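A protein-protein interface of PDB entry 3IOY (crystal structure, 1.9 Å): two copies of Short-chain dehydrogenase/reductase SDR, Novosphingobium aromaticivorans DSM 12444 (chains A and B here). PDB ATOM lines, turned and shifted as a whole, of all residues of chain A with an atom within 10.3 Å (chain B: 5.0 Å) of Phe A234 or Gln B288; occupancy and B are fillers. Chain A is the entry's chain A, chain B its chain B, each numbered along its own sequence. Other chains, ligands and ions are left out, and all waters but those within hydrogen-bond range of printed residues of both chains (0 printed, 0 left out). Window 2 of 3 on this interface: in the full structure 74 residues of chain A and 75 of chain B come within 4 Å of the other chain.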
ATOM      1  N   GLY A 196       7.232 -12.607   5.625  1.00  0.00           N
ATOM      2  CA  GLY A 196       7.801 -11.288   5.444  1.00  0.00           C
ATOM      3  C   GLY A 196       7.279 -10.399   6.556  1.00  0.00           C
ATOM      4  O   GLY A 196       7.136 -10.830   7.692  1.00  0.00           O
ATOM      5  N   LEU A 197       6.970  -9.161   6.211  1.00  0.00           N
ATOM      6  CA  LEU A 197       6.507  -8.154   7.166  1.00  0.00           C
ATOM      7  C   LEU A 197       5.180  -8.478   7.837  1.00  0.00           C
ATOM      8  O   LEU A 197       4.159  -8.674   7.164  1.00  0.00           O
ATOM      9  CB  LEU A 197       6.357  -6.810   6.446  1.00  0.00           C
ATOM     10  CG  LEU A 197       7.468  -5.780   6.531  1.00  0.00           C
ATOM     11  CD1 LEU A 197       6.885  -4.418   6.065  1.00  0.00           C
ATOM     12  CD2 LEU A 197       8.072  -5.663   7.957  1.00  0.00           C
ATOM     13  N   VAL A 198       5.220  -8.499   9.167  1.00  0.00           N
ATOM     14  CA  VAL A 198       4.069  -8.749  10.008  1.00  0.00           C
ATOM     15  C   VAL A 198       3.608  -7.406  10.564  1.00  0.00           C
ATOM     16  O   VAL A 198       4.444  -6.561  10.854  1.00  0.00           O
ATOM     17  CB  VAL A 198       4.465  -9.649  11.164  1.00  0.00           C
ATOM     18  CG1 VAL A 198       3.246  -9.978  12.020  1.00  0.00           C
ATOM     19  CG2 VAL A 198       5.119 -10.903  10.629  1.00  0.00           C
ATOM     20  N   LYS A 199       2.294  -7.207  10.712  1.00  0.00           N
ATOM     21  CA  LYS A 199       1.743  -5.882  11.079  1.00  0.00           C
ATOM     22  C   LYS A 199       2.300  -5.307  12.395  1.00  0.00           C
ATOM     23  O   LYS A 199       2.348  -6.006  13.413  1.00  0.00           O
ATOM     24  CB  LYS A 199       0.209  -5.894  11.120  1.00  0.00           C
ATOM     25  CG  LYS A 199      -0.356  -4.540  11.589  1.00  0.00           C
ATOM     26  CD  LYS A 199      -1.869  -4.477  11.613  1.00  0.00           C
ATOM     27  CE  LYS A 199      -2.446  -3.471  10.595  1.00  0.00           C
ATOM     28  NZ  LYS A 199      -2.946  -4.112   9.329  1.00  0.00           N
ATOM     29  N   ALA A 229       7.554   6.076   7.593  1.00  0.00           N
ATOM     30  CA  ALA A 229       7.123   5.714   6.237  1.00  0.00           C
ATOM     31  C   ALA A 229       5.839   4.861   6.214  1.00  0.00           C
ATOM     32  O   ALA A 229       5.329   4.507   5.137  1.00  0.00           O
ATOM     33  CB  ALA A 229       8.249   5.001   5.496  1.00  0.00           C
ATOM     34  N   GLY A 230       5.317   4.544   7.401  1.00  0.00           N
ATOM     35  CA  GLY A 230       4.097   3.743   7.540  1.00  0.00           C
ATOM     36  C   GLY A 230       4.368   2.248   7.445  1.00  0.00           C
ATOM     37  O   GLY A 230       3.436   1.450   7.278  1.00  0.00           O
ATOM     38  N   VAL A 231       5.647   1.876   7.552  1.00  0.00           N
ATOM     39  CA  VAL A 231       6.079   0.480   7.436  1.00  0.00           C
ATOM     40  C   VAL A 231       5.330  -0.415   8.426  1.00  0.00           C
ATOM     41  O   VAL A 231       4.735  -1.426   8.038  1.00  0.00           O
ATOM     42  CB  VAL A 231       7.620   0.341   7.600  1.00  0.00           C
ATOM     43  CG1 VAL A 231       8.049  -1.139   7.650  1.00  0.00           C
ATOM     44  CG2 VAL A 231       8.357   1.083   6.474  1.00  0.00           C
ATOM     45  N   HIS A 232       5.340  -0.004   9.692  1.00  0.00           N
ATOM     46  CA  HIS A 232       4.662  -0.712  10.779  1.00  0.00           C
ATOM     47  C   HIS A 232       3.159  -0.976  10.540  1.00  0.00           C
ATOM     48  O   HIS A 232       2.543  -1.759  11.273  1.00  0.00           O
ATOM     49  CB  HIS A 232       4.876   0.042  12.111  1.00  0.00           C
ATOM     50  CG  HIS A 232       4.393   1.470  12.100  1.00  0.00           C
ATOM     51  ND1 HIS A 232       5.030   2.471  11.395  1.00  0.00           N
ATOM     52  CD2 HIS A 232       3.350   2.063  12.733  1.00  0.00           C
ATOM     53  CE1 HIS A 232       4.394   3.615  11.583  1.00  0.00           C
ATOM     54  NE2 HIS A 232       3.372   3.395  12.392  1.00  0.00           N
ATOM     55  N   GLU A 233       2.606  -0.351   9.490  1.00  0.00           N
ATOM     56  CA  GLU A 233       1.148  -0.293   9.242  1.00  0.00           C
ATOM     57  C   GLU A 233       0.631  -1.303   8.219  1.00  0.00           C
ATOM     58  O   GLU A 233      -0.509  -1.757   8.332  1.00  0.00           O
ATOM     59  CB  GLU A 233       0.723   1.108   8.766  1.00  0.00           C
ATOM     60  CG  GLU A 233       1.239   2.266   9.609  1.00  0.00           C
ATOM     61  CD  GLU A 233       0.235   2.739  10.642  1.00  0.00           C
ATOM     62  OE1 GLU A 233      -0.082   1.966  11.580  1.00  0.00           O
ATOM     63  OE2 GLU A 233      -0.230   3.898  10.515  1.00  0.00           O
ATOM     64  N   PHE A 234       1.441  -1.633   7.216  1.00  0.00           N
ATOM     65  CA  PHE A 234       0.986  -2.510   6.135  1.00  0.00           C
ATOM     66  C   PHE A 234       1.528  -3.946   6.181  1.00  0.00           C
ATOM     67  O   PHE A 234       1.459  -4.651   5.180  1.00  0.00           O
ATOM     68  CB  PHE A 234       1.252  -1.890   4.752  1.00  0.00           C
ATOM     69  CG  PHE A 234       2.658  -1.375   4.562  1.00  0.00           C
ATOM     70  CD1 PHE A 234       2.892  -0.005   4.427  1.00  0.00           C
ATOM     71  CD2 PHE A 234       3.752  -2.253   4.524  1.00  0.00           C
ATOM     72  CE1 PHE A 234       4.198   0.483   4.247  1.00  0.00           C
ATOM     73  CE2 PHE A 234       5.067  -1.776   4.354  1.00  0.00           C
ATOM     74  CZ  PHE A 234       5.294  -0.408   4.206  1.00  0.00           C
ATOM     75  N   GLY A 235       2.070  -4.364   7.325  1.00  0.00           N
ATOM     76  CA  GLY A 235       2.469  -5.765   7.527  1.00  0.00           C
ATOM     77  C   GLY A 235       1.263  -6.709   7.546  1.00  0.00           C
ATOM     78  O   GLY A 235       0.141  -6.256   7.745  1.00  0.00           O
ATOM     79  N   MET A 236       1.481  -8.013   7.341  1.00  0.00           N
ATOM     80  CA  MET A 236       0.368  -8.989   7.310  1.00  0.00           C
ATOM     81  C   MET A 236      -0.216  -9.136   8.707  1.00  0.00           C
ATOM     82  O   MET A 236       0.528  -9.132   9.693  1.00  0.00           O
ATOM     83  CB  MET A 236       0.844 -10.349   6.767  1.00  0.00           C
ATOM     84  CG  MET A 236      -0.275 -11.398   6.527  1.00  0.00           C
ATOM     85  SD  MET A 236       0.304 -12.854   5.672  1.00  0.00           S
ATOM     86  CE  MET A 236       0.559 -12.161   4.056  1.00  0.00           C
ATOM     87  N   GLU A 237      -1.541  -9.248   8.799  1.00  0.00           N
ATOM     88  CA  GLU A 237      -2.213  -9.425  10.087  1.00  0.00           C
ATOM     89  C   GLU A 237      -1.915 -10.820  10.653  1.00  0.00           C
ATOM     90  O   GLU A 237      -2.026 -11.814   9.923  1.00  0.00           O
ATOM     91  CB  GLU A 237      -3.733  -9.264   9.929  1.00  0.00           C
ATOM     92  CG  GLU A 237      -4.227  -7.819   9.790  1.00  0.00           C
ATOM     93  CD  GLU A 237      -4.355  -7.073  11.127  1.00  0.00           C
ATOM     94  OE1 GLU A 237      -4.068  -7.670  12.205  1.00  0.00           O
ATOM     95  OE2 GLU A 237      -4.749  -5.870  11.095  1.00  0.00           O
ATOM     96  N   PRO A 238      -1.551 -10.905  11.958  1.00  0.00           N
ATOM     97  CA  PRO A 238      -1.306 -12.223  12.570  1.00  0.00           C
ATOM     98  C   PRO A 238      -2.413 -13.260  12.341  1.00  0.00           C
ATOM     99  O   PRO A 238      -2.095 -14.445  12.146  1.00  0.00           O
ATOM    100  CB  PRO A 238      -1.127 -11.900  14.050  1.00  0.00           C
ATOM    101  CG  PRO A 238      -0.536 -10.520  14.040  1.00  0.00           C
ATOM    102  CD  PRO A 238      -1.205  -9.805  12.885  1.00  0.00           C
ATOM    103  N   VAL A 240      -4.406 -13.534   9.736  1.00  0.00           N
ATOM    104  CA  VAL A 240      -4.316 -13.971   8.347  1.00  0.00           C
ATOM    105  C   VAL A 240      -3.159 -14.945   8.209  1.00  0.00           C
ATOM    106  O   VAL A 240      -3.282 -15.974   7.537  1.00  0.00           O
ATOM    107  CB  VAL A 240      -4.101 -12.781   7.373  1.00  0.00           C
ATOM    108  CG1 VAL A 240      -3.848 -13.299   5.931  1.00  0.00           C
ATOM    109  CG2 VAL A 240      -5.285 -11.803   7.426  1.00  0.00           C
ATOM    110  N   ILE A 241      -2.019 -14.619   8.830  1.00  0.00           N
ATOM    111  CA  ILE A 241      -0.897 -15.580   8.898  1.00  0.00           C
ATOM    112  C   ILE A 241      -1.342 -16.897   9.569  1.00  0.00           C
ATOM    113  O   ILE A 241      -1.064 -17.976   9.067  1.00  0.00           O
ATOM    114  CB  ILE A 241       0.355 -15.002   9.644  1.00  0.00           C
ATOM    115  CG1 ILE A 241       0.832 -13.717   8.971  1.00  0.00           C
ATOM    116  CG2 ILE A 241       1.487 -16.024   9.627  1.00  0.00           C
ATOM    117  CD1 ILE A 241       2.062 -12.995   9.644  1.00  0.00           C
ATOM    118  N   HIS A 259       3.603 -15.091   2.792  1.00  0.00           N
ATOM    119  CA  HIS A 259       3.640 -13.862   1.979  1.00  0.00           C
ATOM    120  C   HIS A 259       3.963 -14.240   0.532  1.00  0.00           C
ATOM    121  O   HIS A 259       5.003 -14.877   0.257  1.00  0.00           O
ATOM    122  CB  HIS A 259       4.711 -12.882   2.510  1.00  0.00           C
ATOM    123  CG  HIS A 259       4.400 -12.262   3.843  1.00  0.00           C
ATOM    124  ND1 HIS A 259       4.166 -13.006   4.982  1.00  0.00           N
ATOM    125  CD2 HIS A 259       4.340 -10.958   4.230  1.00  0.00           C
ATOM    126  CE1 HIS A 259       3.948 -12.196   6.004  1.00  0.00           C
ATOM    127  NE2 HIS A 259       4.062 -10.946   5.578  1.00  0.00           N
ATOM    128  N   ASP A 261       4.819 -12.121  -1.507  1.00  0.00           N
ATOM    129  CA  ASP A 261       5.691 -10.962  -1.853  1.00  0.00           C
ATOM    130  C   ASP A 261       7.014 -11.297  -2.537  1.00  0.00           C
ATOM    131  O   ASP A 261       7.356 -10.706  -3.564  1.00  0.00           O
ATOM    132  CB  ASP A 261       6.038 -10.111  -0.617  1.00  0.00           C
ATOM    133  CG  ASP A 261       4.860  -9.855   0.296  1.00  0.00           C
ATOM    134  OD1 ASP A 261       3.814 -10.518   0.145  1.00  0.00           O
ATOM    135  OD2 ASP A 261       4.995  -9.004   1.201  1.00  0.00           O
ATOM    136  N   HIS A 262       7.731 -12.277  -1.995  1.00  0.00           N
ATOM    137  CA  HIS A 262       9.137 -12.522  -2.393  1.00  0.00           C
ATOM    138  C   HIS A 262       9.373 -13.552  -3.483  1.00  0.00           C
ATOM    139  O   HIS A 262      10.516 -13.878  -3.801  1.00  0.00           O
ATOM    140  CB  HIS A 262       9.968 -12.879  -1.147  1.00  0.00           C
ATOM    141  CG  HIS A 262       9.772 -11.923  -0.027  1.00  0.00           C
ATOM    142  ND1 HIS A 262       8.832 -12.116   0.958  1.00  0.00           N
ATOM    143  CD2 HIS A 262      10.369 -10.740   0.249  1.00  0.00           C
ATOM    144  CE1 HIS A 262       8.864 -11.100   1.803  1.00  0.00           C
ATOM    145  NE2 HIS A 262       9.789 -10.251   1.397  1.00  0.00           N
ATOM    146  N   PRO B 284      -5.218  -7.327   3.359  1.00  0.00           N
ATOM    147  CA  PRO B 284      -5.203  -5.861   3.543  1.00  0.00           C
ATOM    148  C   PRO B 284      -3.769  -5.300   3.734  1.00  0.00           C
ATOM    149  O   PRO B 284      -3.010  -5.777   4.601  1.00  0.00           O
ATOM    150  CB  PRO B 284      -6.073  -5.647   4.807  1.00  0.00           C
ATOM    151  CG  PRO B 284      -6.069  -6.986   5.513  1.00  0.00           C
ATOM    152  CD  PRO B 284      -6.039  -7.998   4.390  1.00  0.00           C
ATOM    153  N   GLY B 285      -3.407  -4.325   2.901  1.00  0.00           N
ATOM    154  CA  GLY B 285      -2.084  -3.699   2.950  1.00  0.00           C
ATOM    155  C   GLY B 285      -1.120  -4.250   1.917  1.00  0.00           C
ATOM    156  O   GLY B 285      -0.019  -3.721   1.738  1.00  0.00           O
ATOM    157  N   TYR B 286      -1.559  -5.301   1.231  1.00  0.00           N
ATOM    158  CA  TYR B 286      -0.785  -5.976   0.213  1.00  0.00           C
ATOM    159  C   TYR B 286      -0.095  -5.050  -0.800  1.00  0.00           C
ATOM    160  O   TYR B 286       1.088  -5.226  -1.091  1.00  0.00           O
ATOM    161  CB  TYR B 286      -1.668  -6.954  -0.533  1.00  0.00           C
ATOM    162  CG  TYR B 286      -0.945  -7.638  -1.634  1.00  0.00           C
ATOM    163  CD1 TYR B 286      -0.367  -8.891  -1.444  1.00  0.00           C
ATOM    164  CD2 TYR B 286      -0.811  -7.023  -2.880  1.00  0.00           C
ATOM    165  CE1 TYR B 286       0.301  -9.520  -2.467  1.00  0.00           C
ATOM    166  CE2 TYR B 286      -0.138  -7.635  -3.903  1.00  0.00           C
ATOM    167  CZ  TYR B 286       0.419  -8.883  -3.699  1.00  0.00           C
ATOM    168  OH  TYR B 286       1.086  -9.485  -4.741  1.00  0.00           O
ATOM    169  N   ASP B 287      -0.846  -4.100  -1.364  1.00  0.00           N
ATOM    170  CA  ASP B 287      -0.291  -3.216  -2.380  1.00  0.00           C
ATOM    171  C   ASP B 287       0.890  -2.362  -1.870  1.00  0.00           C
ATOM    172  O   ASP B 287       1.951  -2.329  -2.501  1.00  0.00           O
ATOM    173  CB  ASP B 287      -1.398  -2.355  -3.007  1.00  0.00           C
ATOM    174  CG  ASP B 287      -2.182  -3.092  -4.101  1.00  0.00           C
ATOM    175  OD1 ASP B 287      -3.216  -2.530  -4.517  1.00  0.00           O
ATOM    176  OD2 ASP B 287      -1.784  -4.193  -4.568  1.00  0.00           O
ATOM    177  N   GLN B 288       0.715  -1.701  -0.727  1.00  0.00           N
ATOM    178  CA  GLN B 288       1.790  -0.938  -0.091  1.00  0.00           C
ATOM    179  C   GLN B 288       2.968  -1.839   0.284  1.00  0.00           C
ATOM    180  O   GLN B 288       4.102  -1.562  -0.080  1.00  0.00           O
ATOM    181  CB  GLN B 288       1.298  -0.280   1.188  1.00  0.00           C
ATOM    182  CG  GLN B 288       0.236   0.789   1.026  1.00  0.00           C
ATOM    183  CD  GLN B 288      -0.146   1.357   2.383  1.00  0.00           C
ATOM    184  OE1 GLN B 288      -1.059   0.853   3.039  1.00  0.00           O
ATOM    185  NE2 GLN B 288       0.589   2.374   2.834  1.00  0.00           N
ATOM    186  N   ARG B 289       2.678  -2.924   1.002  1.00  0.00           N
ATOM    187  CA  ARG B 289       3.706  -3.872   1.439  1.00  0.00           C
ATOM    188  C   ARG B 289       4.574  -4.404   0.298  1.00  0.00           C
ATOM    189  O   ARG B 289       5.797  -4.464   0.432  1.00  0.00           O
ATOM    190  CB  ARG B 289       3.081  -5.036   2.229  1.00  0.00           C
ATOM    191  CG  ARG B 289       4.100  -5.984   2.833  1.00  0.00           C
ATOM    192  CD  ARG B 289       3.419  -7.085   3.591  1.00  0.00           C
ATOM    193  NE  ARG B 289       2.859  -8.080   2.687  1.00  0.00           N
ATOM    194  CZ  ARG B 289       1.584  -8.452   2.656  1.00  0.00           C
ATOM    195  NH1 ARG B 289       1.193  -9.394   1.794  1.00  0.00           N
ATOM    196  NH2 ARG B 289       0.711  -7.901   3.486  1.00  0.00           N
ATOM    197  N   VAL B 290       3.957  -4.768  -0.819  1.00  0.00           N
ATOM    198  CA  VAL B 290       4.696  -5.316  -1.960  1.00  0.00           C
ATOM    199  C   VAL B 290       5.507  -4.235  -2.687  1.00  0.00           C
ATOM    200  O   VAL B 290       6.554  -4.540  -3.270  1.00  0.00           O
ATOM    201  CB  VAL B 290       3.775  -6.122  -2.921  1.00  0.00           C
ATOM    202  CG1 VAL B 290       4.508  -6.573  -4.199  1.00  0.00           C
ATOM    203  CG2 VAL B 290       3.230  -7.342  -2.193  1.00  0.00           C
ATOM    204  N   ALA B 291       5.026  -2.990  -2.642  1.00  0.00           N
ATOM    205  CA  ALA B 291       5.753  -1.832  -3.204  1.00  0.00           C
ATOM    206  C   ALA B 291       7.037  -1.624  -2.420  1.00  0.00           C
ATOM    207  O   ALA B 291       8.108  -1.411  -2.993  1.00  0.00           O
ATOM    208  CB  ALA B 291       4.907  -0.575  -3.126  1.00  0.00           C
ATOM    209  N   PHE B 292       6.906  -1.683  -1.100  1.00  0.00           N
ATOM    210  CA  PHE B 292       8.041  -1.591  -0.204  1.00  0.00           C
ATOM    211  C   PHE B 292       9.043  -2.746  -0.400  1.00  0.00           C
ATOM    212  O   PHE B 292      10.246  -2.519  -0.428  1.00  0.00           O
ATOM    213  CB  PHE B 292       7.557  -1.526   1.243  1.00  0.00           C
ATOM    214  CG  PHE B 292       8.629  -1.171   2.208  1.00  0.00           C
ATOM    215  CD1 PHE B 292       9.030   0.158   2.360  1.00  0.00           C
ATOM    216  CD2 PHE B 292       9.265  -2.165   2.957  1.00  0.00           C
ATOM    217  CE1 PHE B 292      10.047   0.497   3.259  1.00  0.00           C
ATOM    218  CE2 PHE B 292      10.287  -1.845   3.855  1.00  0.00           C
ATOM    219  CZ  PHE B 292      10.677  -0.511   4.010  1.00  0.00           C
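Phe A234 touches four residues of chain B. Of chain A, only Phe A234 comes within 4 Å of Gln B288. Of chain A, only Phe A234 (3.7 Å) comes within 4 Å of Gly B285. No residue of chain A comes within 4 Å of Asp B287. Arg B289 touches just these residues of chain A: Leu A197, Phe A234, Met A236, His A259 and Asp A261. Ala B291 touches none of the printed residues of chain A. Printed residues of chain B within 4 Å of Met A236: Arg B289 (3.6 Å). Of the printed residues of chain B, His A259 touches Arg B289 (3.6 Å). Of the printed residues of chain B, Leu A197 touches Arg B289 (3.98 Å). Of the printed residues of chain A, Val B290 touches Asp A261. Printed residues of chain B within 4 Å of Val A231: Phe B292 (3.7 Å). Pro B284 touches none of the printed residues of chain A. Pro A238 touches none of the printed residues of chain B. The nearest residue of chain B that does not touch Phe A234 is Pro B284 (4.6 Å). The nearest residue of chain A that does not touch Gln B288 is Gly A230 (5.4 Å).
Among the printed residues, merely in contact across the chains: Leu A197 with Arg B289, Val A231 with Phe B292, Phe A234 with Gly B285, Phe A234 with Gln B288, Phe A234 with Arg B289, Phe A234 with Phe B292, Met A236 with Arg B289, His A259 with Arg B289 and Asp A261 with Val B290.
ND1 of His A259 sits at hydrogen-bond distance from N of Gly A196 (3.2 Å). O of Leu A197 is in hydrogen-bond range of N of Met A236, 2.8 Å away. The backbone carbonyl oxygen (O) of Leu A197 is in hydrogen-bond range of a ring nitrogen (NE2) of His A259 (2.8 Å). The backbone NH (N) of Lys A199 is in hydrogen-bond range of the backbone carbonyl oxygen (O) of Met A236.
Of the 19 printed residues of chain A, 6 touch a printed residue of chain B. Printed residues of chain A that touch a printed residue of chain B: Leu A197, Val A231, Phe A234, Met A236, His A259 and Asp A261. Hydrophobic or aromatic side chains of chain A that line the printed part of chain B: Val A231, Phe A234, Met A236 and His A259. Hydrophobic or aromatic side chains of chain B within 4 Å of the printed part of chain A: Val B290 and Phe B292. Among the printed residues, 10 pairs touch across the chains.
No position is printed for both chains.
OD2 of Asp A261 lies within salt-bridge range of NE of Arg B289, 2.8 Å away.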
